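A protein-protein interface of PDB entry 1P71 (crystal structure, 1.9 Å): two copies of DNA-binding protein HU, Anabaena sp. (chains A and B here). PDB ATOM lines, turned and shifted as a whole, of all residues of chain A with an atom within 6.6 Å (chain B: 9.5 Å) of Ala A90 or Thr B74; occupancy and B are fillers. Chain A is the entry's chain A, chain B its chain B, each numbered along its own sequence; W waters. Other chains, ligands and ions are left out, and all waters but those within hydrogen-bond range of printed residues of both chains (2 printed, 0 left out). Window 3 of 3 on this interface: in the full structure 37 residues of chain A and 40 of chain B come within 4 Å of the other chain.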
ATOM      1  N   PHE A  85      13.595 -19.956   4.072  1.00  0.00           N
ATOM      2  CA  PHE A  85      13.516 -18.517   4.321  1.00  0.00           C
ATOM      3  C   PHE A  85      14.641 -17.767   3.560  1.00  0.00           C
ATOM      4  O   PHE A  85      14.377 -16.829   2.814  1.00  0.00           O
ATOM      5  CB  PHE A  85      13.565 -18.261   5.828  1.00  0.00           C
ATOM      6  CG  PHE A  85      13.018 -16.926   6.252  1.00  0.00           C
ATOM      7  CD1 PHE A  85      12.758 -15.907   5.309  1.00  0.00           C
ATOM      8  CD2 PHE A  85      12.767 -16.674   7.588  1.00  0.00           C
ATOM      9  CE1 PHE A  85      12.256 -14.684   5.718  1.00  0.00           C
ATOM     10  CE2 PHE A  85      12.255 -15.440   8.003  1.00  0.00           C
ATOM     11  CZ  PHE A  85      12.006 -14.443   7.065  1.00  0.00           C
ATOM     12  N   ARG A  86      15.886 -18.201   3.730  1.00  0.00           N
ATOM     13  CA  ARG A  86      17.022 -17.613   2.990  1.00  0.00           C
ATOM     14  C   ARG A  86      16.891 -17.584   1.464  1.00  0.00           C
ATOM     15  O   ARG A  86      17.298 -16.617   0.818  1.00  0.00           O
ATOM     16  CB  ARG A  86      18.334 -18.283   3.384  1.00  0.00           C
ATOM     17  CG  ARG A  86      18.710 -17.999   4.845  1.00  0.00           C
ATOM     18  CD  ARG A  86      19.963 -18.699   5.353  1.00  0.00           C
ATOM     19  NE  ARG A  86      20.247 -19.960   4.660  1.00  0.00           N
ATOM     20  CZ  ARG A  86      20.276 -21.157   5.250  1.00  0.00           C
ATOM     21  NH1 ARG A  86      20.037 -21.268   6.550  1.00  0.00           N
ATOM     22  NH2 ARG A  86      20.552 -22.244   4.532  1.00  0.00           N
ATOM     23  N   GLU A  87      16.340 -18.651   0.899  1.00  0.00           N
ATOM     24  CA  GLU A  87      16.227 -18.813  -0.544  1.00  0.00           C
ATOM     25  C   GLU A  87      15.009 -18.118  -1.160  1.00  0.00           C
ATOM     26  O   GLU A  87      15.014 -17.790  -2.344  1.00  0.00           O
ATOM     27  CB  GLU A  87      16.317 -20.291  -0.926  1.00  0.00           C
ATOM     28  CG  GLU A  87      17.703 -20.887  -0.635  1.00  0.00           C
ATOM     29  CD  GLU A  87      17.908 -22.298  -1.163  1.00  0.00           C
ATOM     30  OE1 GLU A  87      19.079 -22.720  -1.301  1.00  0.00           O
ATOM     31  OE2 GLU A  87      16.913 -22.993  -1.443  1.00  0.00           O
ATOM     32  N   LYS A  88      13.982 -17.861  -0.364  1.00  0.00           N
ATOM     33  CA  LYS A  88      12.867 -17.051  -0.838  1.00  0.00           C
ATOM     34  C   LYS A  88      13.300 -15.580  -0.858  1.00  0.00           C
ATOM     35  O   LYS A  88      12.948 -14.828  -1.765  1.00  0.00           O
ATOM     36  CB  LYS A  88      11.618 -17.249   0.027  1.00  0.00           C
ATOM     37  CG  LYS A  88      10.942 -18.628  -0.064  1.00  0.00           C
ATOM     38  CD  LYS A  88      10.794 -19.185  -1.495  1.00  0.00           C
ATOM     39  CE  LYS A  88       9.495 -18.743  -2.169  1.00  0.00           C
ATOM     40  NZ  LYS A  88       8.585 -19.906  -2.552  1.00  0.00           N
ATOM     41  N   VAL A  89      14.062 -15.185   0.156  1.00  0.00           N
ATOM     42  CA  VAL A  89      14.630 -13.843   0.232  1.00  0.00           C
ATOM     43  C   VAL A  89      15.741 -13.660  -0.818  1.00  0.00           C
ATOM     44  O   VAL A  89      15.868 -12.597  -1.423  1.00  0.00           O
ATOM     45  CB  VAL A  89      15.146 -13.541   1.675  1.00  0.00           C
ATOM     46  CG1 VAL A  89      15.908 -12.238   1.723  1.00  0.00           C
ATOM     47  CG2 VAL A  89      13.996 -13.481   2.630  1.00  0.00           C
ATOM     48  N   ALA A  90      16.524 -14.710  -1.055  1.00  0.00           N
ATOM     49  CA  ALA A  90      17.543 -14.682  -2.102  1.00  0.00           C
ATOM     50  C   ALA A  90      17.550 -15.948  -2.986  1.00  0.00           C
ATOM     51  O   ALA A  90      18.353 -16.866  -2.766  1.00  0.00           O
ATOM     52  CB  ALA A  90      18.930 -14.415  -1.494  1.00  0.00           C
ATOM     53  N   PRO A  91      16.661 -15.988  -3.987  1.00  0.00           N
ATOM     54  CA  PRO A  91      16.555 -17.132  -4.907  1.00  0.00           C
ATOM     55  C   PRO A  91      17.892 -17.534  -5.543  1.00  0.00           C
ATOM     56  O   PRO A  91      18.541 -16.706  -6.217  1.00  0.00           O
ATOM     57  CB  PRO A  91      15.575 -16.632  -5.971  1.00  0.00           C
ATOM     58  CG  PRO A  91      14.731 -15.646  -5.244  1.00  0.00           C
ATOM     59  CD  PRO A  91      15.670 -14.942  -4.316  1.00  0.00           C
ATOM     60  N   PRO A  92      18.293 -18.789  -5.308  1.00  0.00           N
ATOM     61  CA  PRO A  92      19.610 -19.304  -5.717  1.00  0.00           C
ATOM     62  C   PRO A  92      19.955 -19.025  -7.171  1.00  0.00           C
ATOM     63  O   PRO A  92      19.092 -19.170  -8.052  1.00  0.00           O
ATOM     64  CB  PRO A  92      19.481 -20.814  -5.490  1.00  0.00           C
ATOM     65  CG  PRO A  92      18.483 -20.929  -4.379  1.00  0.00           C
ATOM     66  CD  PRO A  92      17.491 -19.815  -4.608  1.00  0.00           C
ATOM     67  N   LYS A  93      21.199 -18.608  -7.406  1.00  0.00           N
ATOM     68  CA  LYS A  93      21.723 -18.446  -8.753  1.00  0.00           C
ATOM     69  C   LYS A  93      22.798 -19.506  -9.035  1.00  0.00           C
ATOM     70  O   LYS A  93      22.801 -20.131 -10.098  1.00  0.00           O
ATOM     71  CB  LYS A  93      22.278 -17.027  -8.972  1.00  0.00           C
ATOM     72  CG  LYS A  93      22.930 -16.844 -10.355  1.00  0.00           C
ATOM     73  CD  LYS A  93      22.671 -15.476 -10.982  1.00  0.00           C
ATOM     74  CE  LYS A  93      23.754 -15.151 -12.009  1.00  0.00           C
ATOM     75  NZ  LYS A  93      24.247 -13.745 -11.883  1.00  0.00           N
ATOM     76  N   ILE B  33       7.492 -15.194   5.746  1.00  0.00           N
ATOM     77  CA  ILE B  33       8.538 -15.432   4.750  1.00  0.00           C
ATOM     78  C   ILE B  33       8.252 -14.679   3.453  1.00  0.00           C
ATOM     79  O   ILE B  33       9.151 -14.088   2.849  1.00  0.00           O
ATOM     80  CB  ILE B  33       8.669 -16.948   4.482  1.00  0.00           C
ATOM     81  CG1 ILE B  33       9.427 -17.623   5.634  1.00  0.00           C
ATOM     82  CG2 ILE B  33       9.358 -17.223   3.141  1.00  0.00           C
ATOM     83  CD1 ILE B  33       9.597 -19.141   5.503  1.00  0.00           C
ATOM     84  N   VAL B  36       8.528 -10.846   4.022  1.00  0.00           N
ATOM     85  CA  VAL B  36       9.942 -10.457   4.046  1.00  0.00           C
ATOM     86  C   VAL B  36      10.597 -10.560   2.672  1.00  0.00           C
ATOM     87  O   VAL B  36      11.296  -9.637   2.250  1.00  0.00           O
ATOM     88  CB  VAL B  36      10.752 -11.235   5.113  1.00  0.00           C
ATOM     89  CG1 VAL B  36      12.244 -10.956   4.963  1.00  0.00           C
ATOM     90  CG2 VAL B  36      10.252 -10.872   6.509  1.00  0.00           C
ATOM     91  N   SER B  37      10.374 -11.676   1.977  1.00  0.00           N
ATOM     92  CA  SER B  37      10.922 -11.864   0.627  1.00  0.00           C
ATOM     93  C   SER B  37      10.500 -10.773  -0.340  1.00  0.00           C
ATOM     94  O   SER B  37      11.233 -10.475  -1.285  1.00  0.00           O
ATOM     95  CB  SER B  37      10.537 -13.228   0.055  1.00  0.00           C
ATOM     96  OG  SER B  37      11.035 -14.260   0.886  1.00  0.00           O
ATOM     97  N   SER B  38       9.336 -10.168  -0.112  1.00  0.00           N
ATOM     98  CA  SER B  38       8.874  -9.099  -1.001  1.00  0.00           C
ATOM     99  C   SER B  38       9.278  -7.703  -0.504  1.00  0.00           C
ATOM    100  O   SER B  38       8.869  -6.694  -1.080  1.00  0.00           O
ATOM    101  CB  SER B  38       7.361  -9.202  -1.238  1.00  0.00           C
ATOM    102  OG  SER B  38       6.646  -8.505  -0.237  1.00  0.00           O
ATOM    103  N   SER B  52      14.225  -7.884   5.509  1.00  0.00           N
ATOM    104  CA  SER B  52      15.280  -8.201   4.564  1.00  0.00           C
ATOM    105  C   SER B  52      16.440  -7.215   4.765  1.00  0.00           C
ATOM    106  O   SER B  52      16.211  -6.015   4.856  1.00  0.00           O
ATOM    107  CB  SER B  52      14.711  -8.022   3.141  1.00  0.00           C
ATOM    108  OG  SER B  52      15.485  -8.671   2.158  1.00  0.00           O
ATOM    109  N   ARG B  53      17.674  -7.721   4.818  1.00  0.00           N
ATOM    110  CA  ARG B  53      18.859  -6.857   4.801  1.00  0.00           C
ATOM    111  C   ARG B  53      19.707  -7.054   3.543  1.00  0.00           C
ATOM    112  O   ARG B  53      19.864  -8.159   3.069  1.00  0.00           O
ATOM    113  CB  ARG B  53      19.704  -7.056   6.050  1.00  0.00           C
ATOM    114  CG  ARG B  53      18.989  -6.613   7.303  1.00  0.00           C
ATOM    115  CD  ARG B  53      19.904  -6.360   8.477  1.00  0.00           C
ATOM    116  NE  ARG B  53      19.149  -5.848   9.619  1.00  0.00           N
ATOM    117  CZ  ARG B  53      19.339  -6.229  10.877  1.00  0.00           C
ATOM    118  NH1 ARG B  53      20.257  -7.149  11.182  1.00  0.00           N
ATOM    119  NH2 ARG B  53      18.588  -5.707  11.835  1.00  0.00           N
ATOM    120  N   GLU B  54      20.214  -5.960   2.995  1.00  0.00           N
ATOM    121  CA  GLU B  54      21.165  -6.015   1.892  1.00  0.00           C
ATOM    122  C   GLU B  54      22.552  -6.328   2.429  1.00  0.00           C
ATOM    123  O   GLU B  54      22.966  -5.832   3.469  1.00  0.00           O
ATOM    124  CB  GLU B  54      21.198  -4.703   1.104  1.00  0.00           C
ATOM    125  CG  GLU B  54      19.853  -4.266   0.538  1.00  0.00           C
ATOM    126  CD  GLU B  54      19.397  -5.068  -0.681  1.00  0.00           C
ATOM    127  OE1 GLU B  54      20.090  -5.051  -1.720  1.00  0.00           O
ATOM    128  OE2 GLU B  54      18.329  -5.711  -0.610  1.00  0.00           O
ATOM    129  N   ARG B  55      23.265  -7.167   1.698  1.00  0.00           N
ATOM    130  CA  ARG B  55      24.637  -7.535   2.018  1.00  0.00           C
ATOM    131  C   ARG B  55      25.416  -7.189   0.761  1.00  0.00           C
ATOM    132  O   ARG B  55      25.031  -7.611  -0.315  1.00  0.00           O
ATOM    133  CB  ARG B  55      24.671  -9.052   2.257  1.00  0.00           C
ATOM    134  CG  ARG B  55      25.752  -9.593   3.164  1.00  0.00           C
ATOM    135  CD  ARG B  55      25.325  -9.755   4.616  1.00  0.00           C
ATOM    136  NE  ARG B  55      24.606  -8.570   5.077  1.00  0.00           N
ATOM    137  CZ  ARG B  55      24.037  -8.423   6.278  1.00  0.00           C
ATOM    138  NH1 ARG B  55      24.096  -9.378   7.180  1.00  0.00           N
ATOM    139  NH2 ARG B  55      23.396  -7.297   6.562  1.00  0.00           N
ATOM    140  N   LYS B  56      26.460  -6.380   0.895  1.00  0.00           N
ATOM    141  CA  LYS B  56      27.379  -6.076  -0.187  1.00  0.00           C
ATOM    142  C   LYS B  56      28.181  -7.340  -0.545  1.00  0.00           C
ATOM    143  O   LYS B  56      28.292  -8.262   0.261  1.00  0.00           O
ATOM    144  CB  LYS B  56      28.337  -4.939   0.244  1.00  0.00           C
ATOM    145  CG  LYS B  56      27.640  -3.584   0.457  1.00  0.00           C
ATOM    146  CD  LYS B  56      28.549  -2.558   1.121  1.00  0.00           C
ATOM    147  CE  LYS B  56      28.301  -1.162   0.585  1.00  0.00           C
ATOM    148  NZ  LYS B  56      26.882  -0.687   0.765  1.00  0.00           N
ATOM    149  N   ALA B  57      28.747  -7.357  -1.747  1.00  0.00           N
ATOM    150  CA  ALA B  57      29.695  -8.378  -2.138  1.00  0.00           C
ATOM    151  C   ALA B  57      30.852  -8.390  -1.162  1.00  0.00           C
ATOM    152  O   ALA B  57      31.227  -7.355  -0.593  1.00  0.00           O
ATOM    153  CB  ALA B  57      30.199  -8.142  -3.557  1.00  0.00           C
ATOM    154  N   ARG B  58      31.421  -9.566  -0.957  1.00  0.00           N
ATOM    155  CA  ARG B  58      32.581  -9.678  -0.080  1.00  0.00           C
ATOM    156  C   ARG B  58      33.483 -10.790  -0.511  1.00  0.00           C
ATOM    157  O   ARG B  58      33.137 -11.573  -1.373  1.00  0.00           O
ATOM    158  CB  ARG B  58      32.157  -9.918   1.348  1.00  0.00           C
ATOM    159  CG  ARG B  58      31.149 -11.005   1.585  1.00  0.00           C
ATOM    160  CD  ARG B  58      30.417 -10.728   2.867  1.00  0.00           C
ATOM    161  NE  ARG B  58      29.590 -11.827   3.325  1.00  0.00           N
ATOM    162  CZ  ARG B  58      30.026 -12.854   4.028  1.00  0.00           C
ATOM    163  NH1 ARG B  58      31.313 -12.959   4.361  1.00  0.00           N
ATOM    164  NH2 ARG B  58      29.156 -13.791   4.395  1.00  0.00           N
ATOM    165  N   ILE B  71      32.117 -13.390  -2.954  1.00  0.00           N
ATOM    166  CA  ILE B  71      30.752 -13.757  -2.617  1.00  0.00           C
ATOM    167  C   ILE B  71      29.871 -12.584  -3.080  1.00  0.00           C
ATOM    168  O   ILE B  71      30.056 -11.463  -2.644  1.00  0.00           O
ATOM    169  CB  ILE B  71      30.651 -14.039  -1.099  1.00  0.00           C
ATOM    170  CG1 ILE B  71      31.569 -15.205  -0.689  1.00  0.00           C
ATOM    171  CG2 ILE B  71      29.207 -14.337  -0.685  1.00  0.00           C
ATOM    172  CD1 ILE B  71      32.019 -15.178   0.809  1.00  0.00           C
ATOM    173  N   PRO B  72      28.940 -12.828  -4.003  1.00  0.00           N
ATOM    174  CA  PRO B  72      28.146 -11.745  -4.580  1.00  0.00           C
ATOM    175  C   PRO B  72      27.246 -11.070  -3.552  1.00  0.00           C
ATOM    176  O   PRO B  72      27.007 -11.595  -2.477  1.00  0.00           O
ATOM    177  CB  PRO B  72      27.311 -12.465  -5.660  1.00  0.00           C
ATOM    178  CG  PRO B  72      28.054 -13.688  -5.931  1.00  0.00           C
ATOM    179  CD  PRO B  72      28.597 -14.124  -4.616  1.00  0.00           C
ATOM    180  N   ALA B  73      26.772  -9.877  -3.882  1.00  0.00           N
ATOM    181  CA  ALA B  73      25.802  -9.197  -3.032  1.00  0.00           C
ATOM    182  C   ALA B  73      24.541 -10.047  -2.953  1.00  0.00           C
ATOM    183  O   ALA B  73      24.232 -10.802  -3.858  1.00  0.00           O
ATOM    184  CB  ALA B  73      25.500  -7.821  -3.572  1.00  0.00           C
ATOM    185  N   THR B  74      23.828  -9.937  -1.847  1.00  0.00           N
ATOM    186  CA  THR B  74      22.632 -10.718  -1.682  1.00  0.00           C
ATOM    187  C   THR B  74      21.685  -9.978  -0.743  1.00  0.00           C
ATOM    188  O   THR B  74      21.907  -8.795  -0.447  1.00  0.00           O
ATOM    189  CB  THR B  74      23.003 -12.169  -1.170  1.00  0.00           C
ATOM    190  OG1 THR B  74      21.832 -12.990  -1.184  1.00  0.00           O
ATOM    191  CG2 THR B  74      23.557 -12.208   0.292  1.00  0.00           C
ATOM    192  N   ARG B  75      20.617 -10.666  -0.337  1.00  0.00           N
ATOM    193  CA  ARG B  75      19.668 -10.198   0.672  1.00  0.00           C
ATOM    194  C   ARG B  75      19.539 -11.322   1.678  1.00  0.00           C
ATOM    195  O   ARG B  75      19.577 -12.487   1.297  1.00  0.00           O
ATOM    196  CB  ARG B  75      18.292  -9.908   0.032  1.00  0.00           C
ATOM    197  CG  ARG B  75      18.286  -8.731  -0.916  1.00  0.00           C
ATOM    198  CD  ARG B  75      16.936  -8.486  -1.630  1.00  0.00           C
ATOM    199  NE  ARG B  75      17.069  -7.634  -2.819  1.00  0.00           N
ATOM    200  CZ  ARG B  75      16.098  -7.454  -3.719  1.00  0.00           C
ATOM    201  NH1 ARG B  75      14.926  -8.055  -3.581  1.00  0.00           N
ATOM    202  NH2 ARG B  75      16.296  -6.681  -4.766  1.00  0.00           N
ATOM    203  N   VAL B  76      19.403 -10.980   2.962  1.00  0.00           N
ATOM    204  CA  VAL B  76      19.268 -11.978   4.015  1.00  0.00           C
ATOM    205  C   VAL B  76      18.139 -11.562   4.985  1.00  0.00           C
ATOM    206  O   VAL B  76      17.893 -10.360   5.214  1.00  0.00           O
ATOM    207  CB  VAL B  76      20.596 -12.181   4.821  1.00  0.00           C
ATOM    208  CG1 VAL B  76      21.746 -12.681   3.926  1.00  0.00           C
ATOM    209  CG2 VAL B  76      20.985 -10.899   5.542  1.00  0.00           C
ATOM    210  N   PRO B  77      17.412 -12.536   5.517  1.00  0.00           N
ATOM    211  CA  PRO B  77      16.409 -12.229   6.532  1.00  0.00           C
ATOM    212  C   PRO B  77      17.056 -11.907   7.873  1.00  0.00           C
ATOM    213  O   PRO B  77      18.097 -12.479   8.215  1.00  0.00           O
ATOM    214  CB  PRO B  77      15.578 -13.517   6.620  1.00  0.00           C
ATOM    215  CG  PRO B  77      16.397 -14.587   6.014  1.00  0.00           C
ATOM    216  CD  PRO B  77      17.443 -13.966   5.148  1.00  0.00           C
HETATM  217  O   HOH W   1      14.165 -10.881  -1.561  1.00  0.00           O
HETATM  218  O   HOH W   2      18.866 -14.922   2.203  1.00  0.00           O
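Ala A90 touches two residues of chain B.
Thr B74 touches just one residue of chain A: Ala A90.
Of chain B, only Val B36 (3.9 Å), Ser B37 (3.2 Å), Ser B52 (3.6 Å), Arg B75 (3.7 Å) and Val B76 (3.9 Å) come within 4 Å of Val A89.
No residue of chain B comes within 4 Å of Pro A91.
Of the printed residues of chain A, Val B36 touches Phe A85 and Val A89.
Of the printed residues of chain A, Arg B75 touches Val A89 and Ala A90.
Of the printed residues of chain A, Ser B52 touches Val A89 (3.6 Å).
Ala B73 touches none of the printed residues of chain A.
The nearest printed residue of chain A that does not touch Arg B75 is Arg A86 (4.7 Å).
No position is printed for both chains.
Printed residues of chain A that touch a printed residue of chain B: Phe A85, Lys A88, Val A89 and Ala A90.
Hydrophobic or aromatic side chains of chain B within 4 Å of the printed part of chain A: Ile B33, Val B36 and Pro B77.
Among the printed residues, 12 pairs touch across the chains.
Among the printed residues, no Asp or Glu carboxylate lies within 4 Å of a Lys or Arg side-chain nitrogen of the other chain.
The backbone carbonyl oxygen (O) of Lys A88 sits close to the side-chain hydroxyl (OG) of Ser B37, at 3.3 Å.
N of Val A89 sits at hydrogen-bond distance from OG of Ser B37, 3.2 Å away.
Water W1 bridges O of Val A89 (2.4 Å) and O of Ser B37 (3.0 Å).
Water W2 lies within hydrogen-bond range of the backbone carbonyl oxygen (O) of Arg A86 (2.7 Å) and the backbone carbonyl oxygen (O) of Arg B75 (2.7 Å).
Among the printed residues, merely in contact across the chains: Ala A90 with Thr B74 (3.2 Å), Ala A90 with Arg B75 (3.5 Å), Val A89 with Ser B52 (3.6 Å), Phe A85 with Pro B77 (3.6 Å), Val A89 with Arg B75 (3.7 Å), Phe A85 with Ile B33 (3.7 Å), Phe A85 with Val B36 (3.8 Å), Lys A88 with Ile B33 (3.8 Å), Val A89 with Val B36 (3.9 Å) and Val A89 with Val B76 (3.9 Å).
The side-chain hydroxyl of Ser B37 is in hydrogen-bond range of the backbone carbonyl oxygen of Ile B33 (2.7 Å).
The backbone NH (N) of Arg B55 sits at hydrogen-bond distance from the backbone carbonyl oxygen (O) of Thr B74 (3.0 Å).
The guanidinium group of Arg B75 lies within salt-bridge range of the side-chain carboxylate of Glu B54 (3.2 Å).
The backbone NH (N) of Arg B53 is in hydrogen-bond range of the backbone carbonyl oxygen (O) of Val B76, 2.7 Å away.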
